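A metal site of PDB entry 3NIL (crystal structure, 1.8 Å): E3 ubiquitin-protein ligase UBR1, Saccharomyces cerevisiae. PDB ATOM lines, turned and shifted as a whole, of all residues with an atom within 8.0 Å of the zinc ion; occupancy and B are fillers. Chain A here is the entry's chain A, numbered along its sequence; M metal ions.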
ATOM      1  N   ARG A  23      33.649   2.129  -1.733  1.00  0.00           N
ATOM      2  CA  ARG A  23      32.433   2.548  -1.052  1.00  0.00           C
ATOM      3  C   ARG A  23      31.282   1.663  -1.479  1.00  0.00           C
ATOM      4  O   ARG A  23      31.228   1.221  -2.621  1.00  0.00           O
ATOM      5  CB  ARG A  23      32.088   3.995  -1.397  1.00  0.00           C
ATOM      6  CG  ARG A  23      33.106   5.018  -0.962  1.00  0.00           C
ATOM      7  CD  ARG A  23      32.691   6.407  -1.475  1.00  0.00           C
ATOM      8  NE  ARG A  23      33.364   7.496  -0.754  1.00  0.00           N
ATOM      9  CZ  ARG A  23      34.611   7.895  -0.988  1.00  0.00           C
ATOM     10  NH1 ARG A  23      35.362   7.298  -1.916  1.00  0.00           N
ATOM     11  NH2 ARG A  23      35.119   8.898  -0.291  1.00  0.00           N
ATOM     12  N   CYS A  24      30.356   1.414  -0.570  1.00  0.00           N
ATOM     13  CA  CYS A  24      29.123   0.739  -0.920  1.00  0.00           C
ATOM     14  C   CYS A  24      27.931   1.563  -0.497  1.00  0.00           C
ATOM     15  O   CYS A  24      27.726   1.832   0.702  1.00  0.00           O
ATOM     16  CB  CYS A  24      29.059  -0.653  -0.290  1.00  0.00           C
ATOM     17  SG  CYS A  24      27.466  -1.454  -0.528  1.00  0.00           S
ATOM     18  N   HIS A  25      27.120   1.923  -1.488  1.00  0.00           N
ATOM     19  CA  HIS A  25      25.928   2.744  -1.258  1.00  0.00           C
ATOM     20  C   HIS A  25      25.009   2.130  -0.208  1.00  0.00           C
ATOM     21  O   HIS A  25      24.482   2.849   0.638  1.00  0.00           O
ATOM     22  CB  HIS A  25      25.193   3.000  -2.571  1.00  0.00           C
ATOM     23  CG  HIS A  25      23.929   3.783  -2.423  1.00  0.00           C
ATOM     24  ND1 HIS A  25      23.920   5.158  -2.239  1.00  0.00           N
ATOM     25  CD2 HIS A  25      22.625   3.401  -2.418  1.00  0.00           C
ATOM     26  CE1 HIS A  25      22.671   5.578  -2.124  1.00  0.00           C
ATOM     27  NE2 HIS A  25      21.868   4.526  -2.238  1.00  0.00           N
ATOM     28  N   GLU A  26      24.833   0.809  -0.243  1.00  0.00           N
ATOM     29  CA  GLU A  26      23.897   0.127   0.663  1.00  0.00           C
ATOM     30  C   GLU A  26      24.454  -0.117   2.067  1.00  0.00           C
ATOM     31  O   GLU A  26      23.762   0.108   3.057  1.00  0.00           O
ATOM     32  CB  GLU A  26      23.392  -1.178   0.045  1.00  0.00           C
ATOM     33  CG  GLU A  26      22.379  -1.013  -1.104  1.00  0.00           C
ATOM     34  CD  GLU A  26      23.019  -0.822  -2.469  1.00  0.00           C
ATOM     35  OE1 GLU A  26      24.252  -0.617  -2.547  1.00  0.00           O
ATOM     36  OE2 GLU A  26      22.294  -0.872  -3.490  1.00  0.00           O
ATOM     37  N   CYS A  27      25.694  -0.603   2.158  1.00  0.00           N
ATOM     38  CA  CYS A  27      26.293  -0.947   3.447  1.00  0.00           C
ATOM     39  C   CYS A  27      26.815   0.237   4.266  1.00  0.00           C
ATOM     40  O   CYS A  27      26.793   0.191   5.498  1.00  0.00           O
ATOM     41  CB  CYS A  27      27.421  -1.955   3.245  1.00  0.00           C
ATOM     42  SG  CYS A  27      26.843  -3.515   2.611  1.00  0.00           S
ATOM     43  N   GLY A  28      27.309   1.265   3.594  1.00  0.00           N
ATOM     44  CA  GLY A  28      27.943   2.389   4.277  1.00  0.00           C
ATOM     45  C   GLY A  28      27.002   3.261   5.073  1.00  0.00           C
ATOM     46  O   GLY A  28      25.953   3.670   4.586  1.00  0.00           O
ATOM     47  N   LEU A  35      36.581   1.151   2.350  1.00  0.00           N
ATOM     48  CA  LEU A  35      37.238  -0.143   2.586  1.00  0.00           C
ATOM     49  C   LEU A  35      38.461  -0.286   1.704  1.00  0.00           C
ATOM     50  O   LEU A  35      38.446   0.094   0.525  1.00  0.00           O
ATOM     51  CB  LEU A  35      36.268  -1.298   2.260  1.00  0.00           C
ATOM     52  CG  LEU A  35      35.106  -1.416   3.249  1.00  0.00           C
ATOM     53  CD1 LEU A  35      33.990  -2.373   2.770  1.00  0.00           C
ATOM     54  CD2 LEU A  35      35.639  -1.863   4.599  1.00  0.00           C
ATOM     55  N   PHE A  40      37.954  -5.357   1.523  1.00  0.00           N
ATOM     56  CA  PHE A  40      36.742  -5.369   0.701  1.00  0.00           C
ATOM     57  C   PHE A  40      36.462  -6.787   0.218  1.00  0.00           C
ATOM     58  O   PHE A  40      37.343  -7.438  -0.354  1.00  0.00           O
ATOM     59  CB  PHE A  40      36.854  -4.407  -0.471  1.00  0.00           C
ATOM     60  CG  PHE A  40      35.665  -4.447  -1.397  1.00  0.00           C
ATOM     61  CD1 PHE A  40      34.549  -3.659  -1.135  1.00  0.00           C
ATOM     62  CD2 PHE A  40      35.673  -5.255  -2.549  1.00  0.00           C
ATOM     63  CE1 PHE A  40      33.445  -3.675  -1.993  1.00  0.00           C
ATOM     64  CE2 PHE A  40      34.573  -5.282  -3.394  1.00  0.00           C
ATOM     65  CZ  PHE A  40      33.450  -4.499  -3.127  1.00  0.00           C
ATOM     66  N   ASN A  41      35.250  -7.260   0.482  1.00  0.00           N
ATOM     67  CA  ASN A  41      34.885  -8.623   0.147  1.00  0.00           C
ATOM     68  C   ASN A  41      33.740  -8.578  -0.848  1.00  0.00           C
ATOM     69  O   ASN A  41      32.615  -8.225  -0.485  1.00  0.00           O
ATOM     70  CB  ASN A  41      34.515  -9.433   1.392  1.00  0.00           C
ATOM     71  CG  ASN A  41      34.325 -10.929   1.096  1.00  0.00           C
ATOM     72  OD1 ASN A  41      34.094 -11.315  -0.050  1.00  0.00           O
ATOM     73  ND2 ASN A  41      34.438 -11.753   2.124  1.00  0.00           N
ATOM     74  N   PRO A  42      34.025  -8.920  -2.118  1.00  0.00           N
ATOM     75  CA  PRO A  42      33.046  -8.796  -3.201  1.00  0.00           C
ATOM     76  C   PRO A  42      31.730  -9.513  -2.885  1.00  0.00           C
ATOM     77  O   PRO A  42      30.661  -9.059  -3.307  1.00  0.00           O
ATOM     78  CB  PRO A  42      33.754  -9.463  -4.396  1.00  0.00           C
ATOM     79  CG  PRO A  42      35.199  -9.213  -4.118  1.00  0.00           C
ATOM     80  CD  PRO A  42      35.328  -9.420  -2.621  1.00  0.00           C
ATOM     81  N   LYS A  43      31.837 -10.606  -2.127  1.00  0.00           N
ATOM     82  CA  LYS A  43      30.682 -11.395  -1.680  1.00  0.00           C
ATOM     83  C   LYS A  43      29.671 -10.629  -0.809  1.00  0.00           C
ATOM     84  O   LYS A  43      28.489 -10.956  -0.797  1.00  0.00           O
ATOM     85  CB  LYS A  43      31.160 -12.611  -0.883  1.00  0.00           C
ATOM     86  CG  LYS A  43      32.015 -13.574  -1.657  1.00  0.00           C
ATOM     87  CD  LYS A  43      32.252 -14.787  -0.786  1.00  0.00           C
ATOM     88  CE  LYS A  43      33.504 -15.494  -1.158  1.00  0.00           C
ATOM     89  NZ  LYS A  43      33.933 -16.312  -0.002  1.00  0.00           N
ATOM     90  N   ASP A  44      30.157  -9.645  -0.062  1.00  0.00           N
ATOM     91  CA  ASP A  44      29.286  -8.835   0.789  1.00  0.00           C
ATOM     92  C   ASP A  44      28.397  -7.891  -0.012  1.00  0.00           C
ATOM     93  O   ASP A  44      27.380  -7.427   0.508  1.00  0.00           O
ATOM     94  CB  ASP A  44      30.120  -7.987   1.760  1.00  0.00           C
ATOM     95  CG  ASP A  44      30.671  -8.788   2.923  1.00  0.00           C
ATOM     96  OD1 ASP A  44      30.121  -9.868   3.248  1.00  0.00           O
ATOM     97  OD2 ASP A  44      31.646  -8.305   3.517  1.00  0.00           O
ATOM     98  N   HIS A  45      28.774  -7.603  -1.251  1.00  0.00           N
ATOM     99  CA  HIS A  45      28.210  -6.478  -2.004  1.00  0.00           C
ATOM    100  C   HIS A  45      27.748  -6.851  -3.425  1.00  0.00           C
ATOM    101  O   HIS A  45      27.539  -5.970  -4.255  1.00  0.00           O
ATOM    102  CB  HIS A  45      29.230  -5.345  -2.048  1.00  0.00           C
ATOM    103  CG  HIS A  45      29.873  -5.069  -0.726  1.00  0.00           C
ATOM    104  ND1 HIS A  45      29.242  -4.374   0.277  1.00  0.00           N
ATOM    105  CD2 HIS A  45      31.091  -5.427  -0.229  1.00  0.00           C
ATOM    106  CE1 HIS A  45      30.030  -4.315   1.335  1.00  0.00           C
ATOM    107  NE2 HIS A  45      31.163  -4.940   1.051  1.00  0.00           N
ATOM    108  N   VAL A  46      27.584  -8.141  -3.680  1.00  0.00           N
ATOM    109  CA  VAL A  46      27.093  -8.667  -4.962  1.00  0.00           C
ATOM    110  C   VAL A  46      25.857  -7.933  -5.518  1.00  0.00           C
ATOM    111  O   VAL A  46      25.798  -7.636  -6.708  1.00  0.00           O
ATOM    112  CB  VAL A  46      26.791 -10.190  -4.845  1.00  0.00           C
ATOM    113  CG1 VAL A  46      26.204 -10.738  -6.144  1.00  0.00           C
ATOM    114  CG2 VAL A  46      28.041 -10.956  -4.491  1.00  0.00           C
ATOM    115  N   ASN A  47      24.905  -7.636  -4.635  1.00  0.00           N
ATOM    116  CA  ASN A  47      23.664  -6.975  -5.030  1.00  0.00           C
ATOM    117  C   ASN A  47      23.652  -5.483  -4.698  1.00  0.00           C
ATOM    118  O   ASN A  47      22.610  -4.843  -4.641  1.00  0.00           O
ATOM    119  CB  ASN A  47      22.469  -7.692  -4.370  1.00  0.00           C
ATOM    120  CG  ASN A  47      22.600  -9.219  -4.427  1.00  0.00           C
ATOM    121  OD1 ASN A  47      22.812  -9.802  -5.489  1.00  0.00           O
ATOM    122  ND2 ASN A  47      22.477  -9.864  -3.265  1.00  0.00           N
ATOM    123  N   HIS A  48      24.838  -4.925  -4.485  1.00  0.00           N
ATOM    124  CA  HIS A  48      24.974  -3.567  -3.986  1.00  0.00           C
ATOM    125  C   HIS A  48      25.644  -2.667  -5.008  1.00  0.00           C
ATOM    126  O   HIS A  48      26.321  -3.143  -5.927  1.00  0.00           O
ATOM    127  CB  HIS A  48      25.775  -3.547  -2.683  1.00  0.00           C
ATOM    128  CG  HIS A  48      25.086  -4.254  -1.551  1.00  0.00           C
ATOM    129  ND1 HIS A  48      25.709  -4.501  -0.348  1.00  0.00           N
ATOM    130  CD2 HIS A  48      23.843  -4.769  -1.443  1.00  0.00           C
ATOM    131  CE1 HIS A  48      24.873  -5.142   0.456  1.00  0.00           C
ATOM    132  NE2 HIS A  48      23.731  -5.310  -0.191  1.00  0.00           N
ATOM    133  N   HIS A  49      25.457  -1.362  -4.824  1.00  0.00           N
ATOM    134  CA  HIS A  49      26.089  -0.348  -5.669  1.00  0.00           C
ATOM    135  C   HIS A  49      27.412   0.083  -5.048  1.00  0.00           C
ATOM    136  O   HIS A  49      27.450   0.806  -4.051  1.00  0.00           O
ATOM    137  CB  HIS A  49      25.148   0.843  -5.847  1.00  0.00           C
ATOM    138  CG  HIS A  49      23.868   0.498  -6.538  1.00  0.00           C
ATOM    139  ND1 HIS A  49      22.833  -0.172  -5.908  1.00  0.00           N
ATOM    140  CD2 HIS A  49      23.454   0.718  -7.805  1.00  0.00           C
ATOM    141  CE1 HIS A  49      21.841  -0.343  -6.759  1.00  0.00           C
ATOM    142  NE2 HIS A  49      22.188   0.183  -7.920  1.00  0.00           N
ATOM    143  N   VAL A  50      28.496  -0.364  -5.660  1.00  0.00           N
ATOM    144  CA  VAL A  50      29.833  -0.144  -5.152  1.00  0.00           C
ATOM    145  C   VAL A  50      30.568   0.778  -6.119  1.00  0.00           C
ATOM    146  O   VAL A  50      30.323   0.772  -7.316  1.00  0.00           O
ATOM    147  CB  VAL A  50      30.575  -1.495  -5.006  1.00  0.00           C
ATOM    148  CG1 VAL A  50      32.064  -1.302  -4.685  1.00  0.00           C
ATOM    149  CG2 VAL A  50      29.889  -2.335  -3.938  1.00  0.00           C
ATOM    150  N   TRP A  71      29.078   0.895   9.235  1.00  0.00           N
ATOM    151  CA  TRP A  71      28.387  -0.049   8.341  1.00  0.00           C
ATOM    152  C   TRP A  71      27.004  -0.461   8.824  1.00  0.00           C
ATOM    153  O   TRP A  71      26.823  -0.774  10.004  1.00  0.00           O
ATOM    154  CB  TRP A  71      29.272  -1.301   8.096  1.00  0.00           C
ATOM    155  CG  TRP A  71      30.629  -0.911   7.677  1.00  0.00           C
ATOM    156  CD1 TRP A  71      31.768  -0.902   8.453  1.00  0.00           C
ATOM    157  CD2 TRP A  71      31.014  -0.390   6.398  1.00  0.00           C
ATOM    158  NE1 TRP A  71      32.832  -0.432   7.722  1.00  0.00           N
ATOM    159  CE2 TRP A  71      32.397  -0.102   6.465  1.00  0.00           C
ATOM    160  CE3 TRP A  71      30.311  -0.140   5.208  1.00  0.00           C
ATOM    161  CZ2 TRP A  71      33.107   0.430   5.376  1.00  0.00           C
ATOM    162  CZ3 TRP A  71      31.007   0.381   4.128  1.00  0.00           C
ATOM    163  CH2 TRP A  71      32.398   0.661   4.217  1.00  0.00           C
ATOM    164  N   SER A  73      25.430  -3.103   7.762  1.00  0.00           N
ATOM    165  CA  SER A  73      25.370  -4.559   7.657  1.00  0.00           C
ATOM    166  C   SER A  73      26.693  -5.148   8.107  1.00  0.00           C
ATOM    167  O   SER A  73      27.738  -4.516   7.928  1.00  0.00           O
ATOM    168  CB  SER A  73      25.092  -5.005   6.208  1.00  0.00           C
ATOM    169  OG  SER A  73      23.857  -4.522   5.705  1.00  0.00           O
ATOM    170  N   PRO A  74      26.677  -6.363   8.673  1.00  0.00           N
ATOM    171  CA  PRO A  74      27.904  -7.103   8.938  1.00  0.00           C
ATOM    172  C   PRO A  74      28.761  -7.229   7.672  1.00  0.00           C
ATOM    173  O   PRO A  74      28.243  -7.623   6.625  1.00  0.00           O
ATOM    174  CB  PRO A  74      27.407  -8.499   9.357  1.00  0.00           C
ATOM    175  CG  PRO A  74      25.967  -8.549   8.914  1.00  0.00           C
ATOM    176  CD  PRO A  74      25.488  -7.150   9.054  1.00  0.00           C
ATOM    177  N   LEU A  75      30.037  -6.849   7.771  1.00  0.00           N
ATOM    178  CA  LEU A  75      31.030  -7.170   6.752  1.00  0.00           C
ATOM    179  C   LEU A  75      31.758  -8.430   7.129  1.00  0.00           C
ATOM    180  O   LEU A  75      31.886  -8.761   8.298  1.00  0.00           O
ATOM    181  CB  LEU A  75      32.076  -6.062   6.591  1.00  0.00           C
ATOM    182  CG  LEU A  75      31.570  -4.662   6.253  1.00  0.00           C
ATOM    183  CD1 LEU A  75      32.763  -3.743   6.070  1.00  0.00           C
ATOM    184  CD2 LEU A  75      30.725  -4.704   4.988  1.00  0.00           C
HETATM  185 ZN    ZN M   1      27.393  -3.503   0.371  1.00  0.00          ZN
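A ring nitrogen (ND1) of His 48 lies close to the backbone carbonyl oxygen (O) of Asp 44, at 3.5 Å.
The side-chain sulfur (SG) of Cys 24 lies close to the backbone NH (N) of Glu 26, 3.5 Å away.
Asp 44 touches the zinc ion (O to ZN, 3.9 Å).
Five residues have an atom within 4 Å of the zinc ion: Cys 24, Cys 27, Asp 44, His 45 and His 48.
The zinc ion is bound by a ring nitrogen (ND1) of His 45, at 2.0 Å.
ND1 of His 48 binds the zinc ion (2.1 Å).
SG of Cys 24 binds the zinc ion (2.2 Å).
The zinc ion is bound by SG of Cys 27, at 2.3 Å.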
